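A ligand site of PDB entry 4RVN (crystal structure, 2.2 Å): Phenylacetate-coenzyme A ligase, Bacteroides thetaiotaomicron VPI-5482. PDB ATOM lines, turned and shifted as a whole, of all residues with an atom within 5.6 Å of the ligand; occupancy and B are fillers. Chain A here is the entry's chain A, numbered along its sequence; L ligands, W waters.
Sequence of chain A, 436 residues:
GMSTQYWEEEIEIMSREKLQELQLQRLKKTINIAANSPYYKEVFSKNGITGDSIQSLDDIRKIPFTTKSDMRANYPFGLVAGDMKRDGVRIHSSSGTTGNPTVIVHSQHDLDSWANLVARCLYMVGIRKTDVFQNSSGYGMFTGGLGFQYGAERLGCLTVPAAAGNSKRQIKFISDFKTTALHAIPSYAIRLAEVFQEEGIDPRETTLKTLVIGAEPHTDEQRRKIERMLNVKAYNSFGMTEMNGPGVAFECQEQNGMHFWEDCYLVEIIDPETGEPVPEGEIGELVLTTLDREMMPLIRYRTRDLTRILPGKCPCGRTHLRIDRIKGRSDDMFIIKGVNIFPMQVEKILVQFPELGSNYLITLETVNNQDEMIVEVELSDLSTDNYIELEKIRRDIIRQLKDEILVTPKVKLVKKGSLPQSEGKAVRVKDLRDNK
The side-chain amide nitrogen (ND2) of Asn 340 lies within hydrogen-bond range of an oxygen (O4) of the ligand (2.8 Å).
An oxygen (O6) of the ligand is in hydrogen-bond range of the side-chain carboxylate of Asp 305 (2.6 Å).
The backbone carbonyl oxygen (O) of Ser 237 sits at hydrogen-bond distance from a nitrogen (N3) of the ligand, 2.8 Å away.
The backbone NH of Thr 241 lies within hydrogen-bond range of an oxygen (O1) of the ligand, 3.1 Å away.
The guanidinium group (NH1) of Arg 329 lies within hydrogen-bond range of an oxygen (O6) of the ligand (3.4 Å).
The backbone NH of Ala 215 is in hydrogen-bond range of a nitrogen (N2) of the ligand (3.3 Å).
The side-chain hydroxyl (OG1) of Thr 241 lies within hydrogen-bond range of an oxygen (O1) of the ligand.
The side-chain amide oxygen (OD1) of Asn 236 sits at hydrogen-bond distance from a nitrogen (N3) of the ligand, 2.8 Å away.
Gly 214 touches the ligand (CA to N3, 3.9 Å).
Glu 216 touches the ligand (C to C9, 3.5 Å).
Pro 217 touches the ligand (N to C9, 3.5 Å).
Phe 238 touches the ligand (CD1 to N2, 3.5 Å).
Gly 239 touches the ligand.
Met 240 touches the ligand (CA to O2, 3.6 Å).
Ile 326 touches the ligand.
CD1 of Ile 335 touches C5 of the ligand (3.6 Å).
Hydrophobic or aromatic side chains within 4 Å of the ligand: Pro 217, Phe 238, Met 240, Ile 326 and Ile 335.
The nearest printed residue that does not touch the ligand is Thr 143 (4.1 Å).
Water W4 lies within hydrogen-bond range of an oxygen (O1) of the ligand (2.7 Å), the side-chain carboxylate of Glu 242 (2.8 Å) and the side-chain amide nitrogen of Asn 340 (3.4 Å).
Water W5 lies within hydrogen-bond range of an oxygen (O3) of the ligand and the backbone NH of Asn 340.
Water W1 bridges an oxygen (O6) of the ligand (2.7 Å) and the guanidinium group of Arg 329 (3.2 Å).
Water W2 lies within hydrogen-bond range of a nitrogen (N4) of the ligand (2.8 Å), the side-chain amide nitrogen (ND2) of Asn 236 (3.0 Å) and the backbone NH (N) of Ile 326 (3.1 Å).
Water W3 bridges O1 of the ligand (3.1 Å) and OG1 of Thr 241 (3.1 Å).
The side-chain amide nitrogen of Asn 236 lies close to the side-chain sulfur of Met 258.
O of Glu 216 is in hydrogen-bond range of ND1 of His 218, 3.2 Å away.
The side-chain carboxylate (OE1) of Glu 216 is in hydrogen-bond range of the backbone NH (N) of Gly 338 (3.4 Å).
O of Met 240 sits at hydrogen-bond distance from N of Gly 245 (2.9 Å).
The guanidinium group (NH2) of Arg 329 is in hydrogen-bond range of the backbone carbonyl oxygen (O) of Thr 303.
OD1 of Asp 305 is in salt-bridge range of NH1 of Arg 329, at 2.8 Å.
The side-chain hydroxyl (OG1) of Thr 303 sits close to the backbone NH (N) of Asp 305 (3.1 Å).
The backbone NH (N) of Ser 237 sits at hydrogen-bond distance from the backbone carbonyl oxygen (O) of Ile 213 (2.8 Å).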
ATOM      1  N   THR A 143      32.985  -1.419   9.092  1.00  0.00           N
ATOM      2  CA  THR A 143      33.638  -0.105   9.226  1.00  0.00           C
ATOM      3  C   THR A 143      32.733   0.918   9.952  1.00  0.00           C
ATOM      4  O   THR A 143      33.264   1.865  10.518  1.00  0.00           O
ATOM      5  CB  THR A 143      34.070   0.416   7.862  1.00  0.00           C
ATOM      6  OG1 THR A 143      32.943   0.475   6.963  1.00  0.00           O
ATOM      7  CG2 THR A 143      35.154  -0.442   7.241  1.00  0.00           C
ATOM      8  N   ILE A 213      21.834   8.589   9.394  1.00  0.00           N
ATOM      9  CA  ILE A 213      21.334   7.406   8.702  1.00  0.00           C
ATOM     10  C   ILE A 213      22.094   7.190   7.387  1.00  0.00           C
ATOM     11  O   ILE A 213      22.346   8.134   6.640  1.00  0.00           O
ATOM     12  CB  ILE A 213      19.790   7.470   8.469  1.00  0.00           C
ATOM     13  CG1 ILE A 213      19.346   8.729   7.669  1.00  0.00           C
ATOM     14  CG2 ILE A 213      19.033   7.359   9.807  1.00  0.00           C
ATOM     15  CD1 ILE A 213      17.857   8.797   7.291  1.00  0.00           C
ATOM     16  N   GLY A 214      22.426   5.929   7.106  1.00  0.00           N
ATOM     17  CA  GLY A 214      23.115   5.539   5.890  1.00  0.00           C
ATOM     18  C   GLY A 214      23.180   4.045   5.650  1.00  0.00           C
ATOM     19  O   GLY A 214      22.271   3.316   6.058  1.00  0.00           O
ATOM     20  N   ALA A 215      24.235   3.595   4.917  1.00  0.00           N
ATOM     21  CA  ALA A 215      24.580   2.204   4.575  1.00  0.00           C
ATOM     22  C   ALA A 215      23.713   1.622   3.453  1.00  0.00           C
ATOM     23  O   ALA A 215      24.099   0.611   2.863  1.00  0.00           O
ATOM     24  CB  ALA A 215      24.494   1.284   5.795  1.00  0.00           C
ATOM     25  N   GLU A 216      22.543   2.218   3.155  1.00  0.00           N
ATOM     26  CA  GLU A 216      21.634   1.694   2.149  1.00  0.00           C
ATOM     27  C   GLU A 216      20.777   2.804   1.531  1.00  0.00           C
ATOM     28  O   GLU A 216      20.502   3.801   2.193  1.00  0.00           O
ATOM     29  CB  GLU A 216      20.723   0.591   2.741  1.00  0.00           C
ATOM     30  CG  GLU A 216      19.802   1.004   3.885  1.00  0.00           C
ATOM     31  CD  GLU A 216      18.981  -0.119   4.485  1.00  0.00           C
ATOM     32  OE1 GLU A 216      19.140  -1.284   4.049  1.00  0.00           O
ATOM     33  OE2 GLU A 216      18.171   0.167   5.410  1.00  0.00           O
ATOM     34  N   PRO A 217      20.303   2.618   0.272  1.00  0.00           N
ATOM     35  CA  PRO A 217      19.445   3.643  -0.360  1.00  0.00           C
ATOM     36  C   PRO A 217      18.130   3.861   0.390  1.00  0.00           C
ATOM     37  O   PRO A 217      17.564   2.906   0.945  1.00  0.00           O
ATOM     38  CB  PRO A 217      19.168   3.068  -1.753  1.00  0.00           C
ATOM     39  CG  PRO A 217      20.292   2.120  -2.004  1.00  0.00           C
ATOM     40  CD  PRO A 217      20.555   1.502  -0.662  1.00  0.00           C
ATOM     41  N   HIS A 218      17.666   5.117   0.415  1.00  0.00           N
ATOM     42  CA  HIS A 218      16.394   5.544   1.010  1.00  0.00           C
ATOM     43  C   HIS A 218      15.975   6.889   0.440  1.00  0.00           C
ATOM     44  O   HIS A 218      16.834   7.708   0.115  1.00  0.00           O
ATOM     45  CB  HIS A 218      16.489   5.626   2.546  1.00  0.00           C
ATOM     46  CG  HIS A 218      17.472   6.635   3.049  1.00  0.00           C
ATOM     47  ND1 HIS A 218      18.824   6.370   3.082  1.00  0.00           N
ATOM     48  CD2 HIS A 218      17.252   7.870   3.565  1.00  0.00           C
ATOM     49  CE1 HIS A 218      19.395   7.446   3.594  1.00  0.00           C
ATOM     50  NE2 HIS A 218      18.483   8.376   3.895  1.00  0.00           N
ATOM     51  N   ASN A 236      21.693  12.210   5.955  1.00  0.00           N
ATOM     52  CA  ASN A 236      22.199  11.152   5.085  1.00  0.00           C
ATOM     53  C   ASN A 236      23.718  11.058   5.194  1.00  0.00           C
ATOM     54  O   ASN A 236      24.426  12.054   5.053  1.00  0.00           O
ATOM     55  CB  ASN A 236      21.758  11.387   3.631  1.00  0.00           C
ATOM     56  CG  ASN A 236      21.794  10.162   2.748  1.00  0.00           C
ATOM     57  OD1 ASN A 236      22.146   9.058   3.183  1.00  0.00           O
ATOM     58  ND2 ASN A 236      21.391  10.310   1.495  1.00  0.00           N
ATOM     59  N   SER A 237      24.202   9.838   5.508  1.00  0.00           N
ATOM     60  CA  SER A 237      25.607   9.488   5.712  1.00  0.00           C
ATOM     61  C   SER A 237      26.084   8.485   4.674  1.00  0.00           C
ATOM     62  O   SER A 237      25.587   7.363   4.626  1.00  0.00           O
ATOM     63  CB  SER A 237      25.788   8.900   7.108  1.00  0.00           C
ATOM     64  OG  SER A 237      27.118   8.460   7.351  1.00  0.00           O
ATOM     65  N   PHE A 238      27.076   8.879   3.871  1.00  0.00           N
ATOM     66  CA  PHE A 238      27.605   7.999   2.827  1.00  0.00           C
ATOM     67  C   PHE A 238      29.027   7.559   3.121  1.00  0.00           C
ATOM     68  O   PHE A 238      29.869   8.346   3.548  1.00  0.00           O
ATOM     69  CB  PHE A 238      27.557   8.690   1.455  1.00  0.00           C
ATOM     70  CG  PHE A 238      28.096   7.849   0.319  1.00  0.00           C
ATOM     71  CD1 PHE A 238      27.349   6.794  -0.196  1.00  0.00           C
ATOM     72  CD2 PHE A 238      29.339   8.116  -0.238  1.00  0.00           C
ATOM     73  CE1 PHE A 238      27.856   5.990  -1.225  1.00  0.00           C
ATOM     74  CE2 PHE A 238      29.839   7.318  -1.273  1.00  0.00           C
ATOM     75  CZ  PHE A 238      29.094   6.272  -1.766  1.00  0.00           C
ATOM     76  N   GLY A 239      29.269   6.281   2.837  1.00  0.00           N
ATOM     77  CA  GLY A 239      30.574   5.655   2.965  1.00  0.00           C
ATOM     78  C   GLY A 239      30.669   4.280   2.323  1.00  0.00           C
ATOM     79  O   GLY A 239      29.677   3.724   1.866  1.00  0.00           O
ATOM     80  N   MET A 240      31.902   3.747   2.291  1.00  0.00           N
ATOM     81  CA  MET A 240      32.224   2.408   1.803  1.00  0.00           C
ATOM     82  C   MET A 240      33.580   2.034   2.370  1.00  0.00           C
ATOM     83  O   MET A 240      34.436   2.904   2.545  1.00  0.00           O
ATOM     84  CB  MET A 240      32.179   2.284   0.266  1.00  0.00           C
ATOM     85  CG  MET A 240      33.345   2.926  -0.475  1.00  0.00           C
ATOM     86  SD  MET A 240      33.116   2.849  -2.383  1.00  0.00           S
ATOM     87  CE  MET A 240      31.693   4.075  -2.504  1.00  0.00           C
ATOM     88  N   THR A 241      33.770   0.748   2.684  1.00  0.00           N
ATOM     89  CA  THR A 241      34.984   0.189   3.269  1.00  0.00           C
ATOM     90  C   THR A 241      36.222   0.632   2.467  1.00  0.00           C
ATOM     91  O   THR A 241      37.196   1.107   3.072  1.00  0.00           O
ATOM     92  CB  THR A 241      34.877  -1.335   3.315  1.00  0.00           C
ATOM     93  OG1 THR A 241      33.663  -1.661   4.006  1.00  0.00           O
ATOM     94  CG2 THR A 241      36.075  -2.004   3.976  1.00  0.00           C
ATOM     95  N   GLU A 242      36.172   0.541   1.118  1.00  0.00           N
ATOM     96  CA  GLU A 242      37.267   0.901   0.221  1.00  0.00           C
ATOM     97  C   GLU A 242      37.753   2.331   0.446  1.00  0.00           C
ATOM     98  O   GLU A 242      38.934   2.624   0.270  1.00  0.00           O
ATOM     99  CB  GLU A 242      36.841   0.747  -1.251  1.00  0.00           C
ATOM    100  CG  GLU A 242      36.526  -0.683  -1.691  1.00  0.00           C
ATOM    101  CD  GLU A 242      35.178  -1.260  -1.294  1.00  0.00           C
ATOM    102  OE1 GLU A 242      34.362  -0.547  -0.663  1.00  0.00           O
ATOM    103  OE2 GLU A 242      34.939  -2.428  -1.644  1.00  0.00           O
ATOM    104  N   GLY A 245      35.252   3.860   5.183  1.00  0.00           N
ATOM    105  CA  GLY A 245      33.941   3.499   5.720  1.00  0.00           C
ATOM    106  C   GLY A 245      33.141   4.775   5.852  1.00  0.00           C
ATOM    107  O   GLY A 245      33.050   5.515   4.875  1.00  0.00           O
ATOM    108  N   MET A 258      24.872  15.559  -0.456  1.00  0.00           N
ATOM    109  CA  MET A 258      25.912  15.158   0.478  1.00  0.00           C
ATOM    110  C   MET A 258      27.260  15.732   0.064  1.00  0.00           C
ATOM    111  O   MET A 258      27.764  15.405  -1.021  1.00  0.00           O
ATOM    112  CB  MET A 258      25.989  13.620   0.573  1.00  0.00           C
ATOM    113  CG  MET A 258      24.786  13.006   1.276  1.00  0.00           C
ATOM    114  SD  MET A 258      24.886  11.092   1.370  1.00  0.00           S
ATOM    115  CE  MET A 258      24.581  10.618  -0.474  1.00  0.00           C
ATOM    116  N   THR A 303      33.256   2.165  -8.017  1.00  0.00           N
ATOM    117  CA  THR A 303      32.395   1.862  -6.863  1.00  0.00           C
ATOM    118  C   THR A 303      31.141   1.071  -7.239  1.00  0.00           C
ATOM    119  O   THR A 303      30.568   0.385  -6.399  1.00  0.00           O
ATOM    120  CB  THR A 303      31.976   3.164  -6.181  1.00  0.00           C
ATOM    121  OG1 THR A 303      31.067   3.892  -7.032  1.00  0.00           O
ATOM    122  CG2 THR A 303      33.162   4.050  -5.810  1.00  0.00           C
ATOM    123  N   ASP A 305      28.426   2.451  -7.805  1.00  0.00           N
ATOM    124  CA  ASP A 305      27.367   3.315  -7.283  1.00  0.00           C
ATOM    125  C   ASP A 305      26.969   4.370  -8.311  1.00  0.00           C
ATOM    126  O   ASP A 305      27.847   5.028  -8.869  1.00  0.00           O
ATOM    127  CB  ASP A 305      27.797   4.010  -5.983  1.00  0.00           C
ATOM    128  CG  ASP A 305      27.902   3.103  -4.780  1.00  0.00           C
ATOM    129  OD1 ASP A 305      27.170   2.080  -4.747  1.00  0.00           O
ATOM    130  OD2 ASP A 305      28.629   3.450  -3.838  1.00  0.00           O
ATOM    131  N   ILE A 326      22.188   7.988  -3.497  1.00  0.00           N
ATOM    132  CA  ILE A 326      22.557   6.788  -4.260  1.00  0.00           C
ATOM    133  C   ILE A 326      21.303   5.923  -4.344  1.00  0.00           C
ATOM    134  O   ILE A 326      20.893   5.356  -3.335  1.00  0.00           O
ATOM    135  CB  ILE A 326      23.763   6.004  -3.646  1.00  0.00           C
ATOM    136  CG1 ILE A 326      24.933   6.899  -3.142  1.00  0.00           C
ATOM    137  CG2 ILE A 326      24.206   4.804  -4.512  1.00  0.00           C
ATOM    138  CD1 ILE A 326      25.736   7.682  -4.119  1.00  0.00           C
ATOM    139  N   ARG A 329      22.800   0.668  -8.258  1.00  0.00           N
ATOM    140  CA  ARG A 329      24.142   0.290  -8.695  1.00  0.00           C
ATOM    141  C   ARG A 329      24.170  -0.278 -10.111  1.00  0.00           C
ATOM    142  O   ARG A 329      23.149  -0.760 -10.628  1.00  0.00           O
ATOM    143  CB  ARG A 329      24.731  -0.750  -7.732  1.00  0.00           C
ATOM    144  CG  ARG A 329      25.179  -0.153  -6.411  1.00  0.00           C
ATOM    145  CD  ARG A 329      25.597  -1.221  -5.428  1.00  0.00           C
ATOM    146  NE  ARG A 329      26.843  -1.913  -5.798  1.00  0.00           N
ATOM    147  CZ  ARG A 329      28.047  -1.579  -5.364  1.00  0.00           C
ATOM    148  NH1 ARG A 329      28.209  -0.532  -4.554  1.00  0.00           N
ATOM    149  NH2 ARG A 329      29.111  -2.281  -5.722  1.00  0.00           N
ATOM    150  N   MET A 333      24.974  -6.323  -7.016  1.00  0.00           N
ATOM    151  CA  MET A 333      24.998  -6.282  -5.551  1.00  0.00           C
ATOM    152  C   MET A 333      23.699  -5.694  -4.985  1.00  0.00           C
ATOM    153  O   MET A 333      23.131  -4.764  -5.559  1.00  0.00           O
ATOM    154  CB  MET A 333      26.195  -5.440  -5.065  1.00  0.00           C
ATOM    155  CG  MET A 333      26.663  -5.836  -3.664  1.00  0.00           C
ATOM    156  SD  MET A 333      28.026  -4.655  -2.945  1.00  0.00           S
ATOM    157  CE  MET A 333      26.849  -3.126  -2.510  1.00  0.00           C
ATOM    158  N   ILE A 335      21.674  -4.605  -1.089  1.00  0.00           N
ATOM    159  CA  ILE A 335      21.889  -4.247   0.315  1.00  0.00           C
ATOM    160  C   ILE A 335      20.614  -4.575   1.110  1.00  0.00           C
ATOM    161  O   ILE A 335      19.514  -4.158   0.737  1.00  0.00           O
ATOM    162  CB  ILE A 335      22.302  -2.753   0.452  1.00  0.00           C
ATOM    163  CG1 ILE A 335      23.501  -2.420  -0.472  1.00  0.00           C
ATOM    164  CG2 ILE A 335      22.611  -2.415   1.922  1.00  0.00           C
ATOM    165  CD1 ILE A 335      23.803  -0.946  -0.652  1.00  0.00           C
ATOM    166  N   GLY A 338      21.546  -2.978   5.743  1.00  0.00           N
ATOM    167  CA  GLY A 338      22.786  -2.216   5.605  1.00  0.00           C
ATOM    168  C   GLY A 338      24.014  -3.041   5.248  1.00  0.00           C
ATOM    169  O   GLY A 338      25.125  -2.496   5.202  1.00  0.00           O
ATOM    170  N   ASN A 340      26.077  -5.472   2.501  1.00  0.00           N
ATOM    171  CA  ASN A 340      26.293  -5.727   1.071  1.00  0.00           C
ATOM    172  C   ASN A 340      26.394  -7.219   0.796  1.00  0.00           C
ATOM    173  O   ASN A 340      27.169  -7.917   1.452  1.00  0.00           O
ATOM    174  CB  ASN A 340      27.568  -5.011   0.596  1.00  0.00           C
ATOM    175  CG  ASN A 340      27.605  -3.512   0.819  1.00  0.00           C
ATOM    176  OD1 ASN A 340      26.638  -2.894   1.273  1.00  0.00           O
ATOM    177  ND2 ASN A 340      28.740  -2.913   0.488  1.00  0.00           N
HETATM  178  P1  LIG L   1      30.118  -0.937   2.925  1.00  0.00           P
HETATM  179  O1  LIG L   1      31.392  -1.182   2.195  1.00  0.00           O
HETATM  180  O2  LIG L   1      30.235   0.269   3.897  1.00  0.00           O
HETATM  181  O3  LIG L   1      29.596  -2.173   3.671  1.00  0.00           O
HETATM  182  O4  LIG L   1      28.944  -0.534   1.868  1.00  0.00           O
HETATM  183  C1  LIG L   1      29.074   0.630   1.040  1.00  0.00           C
HETATM  184  C2  LIG L   1      27.938   0.743   0.049  1.00  0.00           C
HETATM  185  O5  LIG L   1      26.706   1.015   0.742  1.00  0.00           O
HETATM  186  C3  LIG L   1      28.098   1.904  -0.924  1.00  0.00           C
HETATM  187  O6  LIG L   1      28.929   1.553  -2.027  1.00  0.00           O
HETATM  188  C4  LIG L   1      26.656   2.181  -1.335  1.00  0.00           C
HETATM  189  O7  LIG L   1      26.211   1.292  -2.354  1.00  0.00           O
HETATM  190  C5  LIG L   1      25.904   1.903  -0.015  1.00  0.00           C
HETATM  191  N1  LIG L   1      25.634   3.098   0.789  1.00  0.00           N
HETATM  192  C6  LIG L   1      26.397   3.608   1.801  1.00  0.00           C
HETATM  193  N2  LIG L   1      25.949   4.739   2.304  1.00  0.00           N
HETATM  194  C7  LIG L   1      24.804   4.987   1.548  1.00  0.00           C
HETATM  195  C8  LIG L   1      23.897   6.061   1.555  1.00  0.00           C
HETATM  196  N3  LIG L   1      23.936   7.071   2.426  1.00  0.00           N
HETATM  197  N4  LIG L   1      22.893   6.041   0.636  1.00  0.00           N
HETATM  198  C9  LIG L   1      22.818   4.999  -0.208  1.00  0.00           C
HETATM  199  N5  LIG L   1      23.613   3.929  -0.292  1.00  0.00           N
HETATM  200  C10 LIG L   1      24.602   3.982   0.618  1.00  0.00           C
HETATM  201  O   HOH W   1      30.467  -0.683  -2.295  1.00  0.00           O
HETATM  202  O   HOH W   2      21.373   8.117  -0.530  1.00  0.00           O
HETATM  203  O   HOH W   3      32.114  -4.116   2.901  1.00  0.00           O
HETATM  204  O   HOH W   4      31.888  -1.884  -0.349  1.00  0.00           O
HETATM  205  O   HOH W   5      28.377  -4.543   4.208  1.00  0.00           O
HETATM  206  O   HOH W   6      23.652   1.801  -2.689  1.00  0.00           O
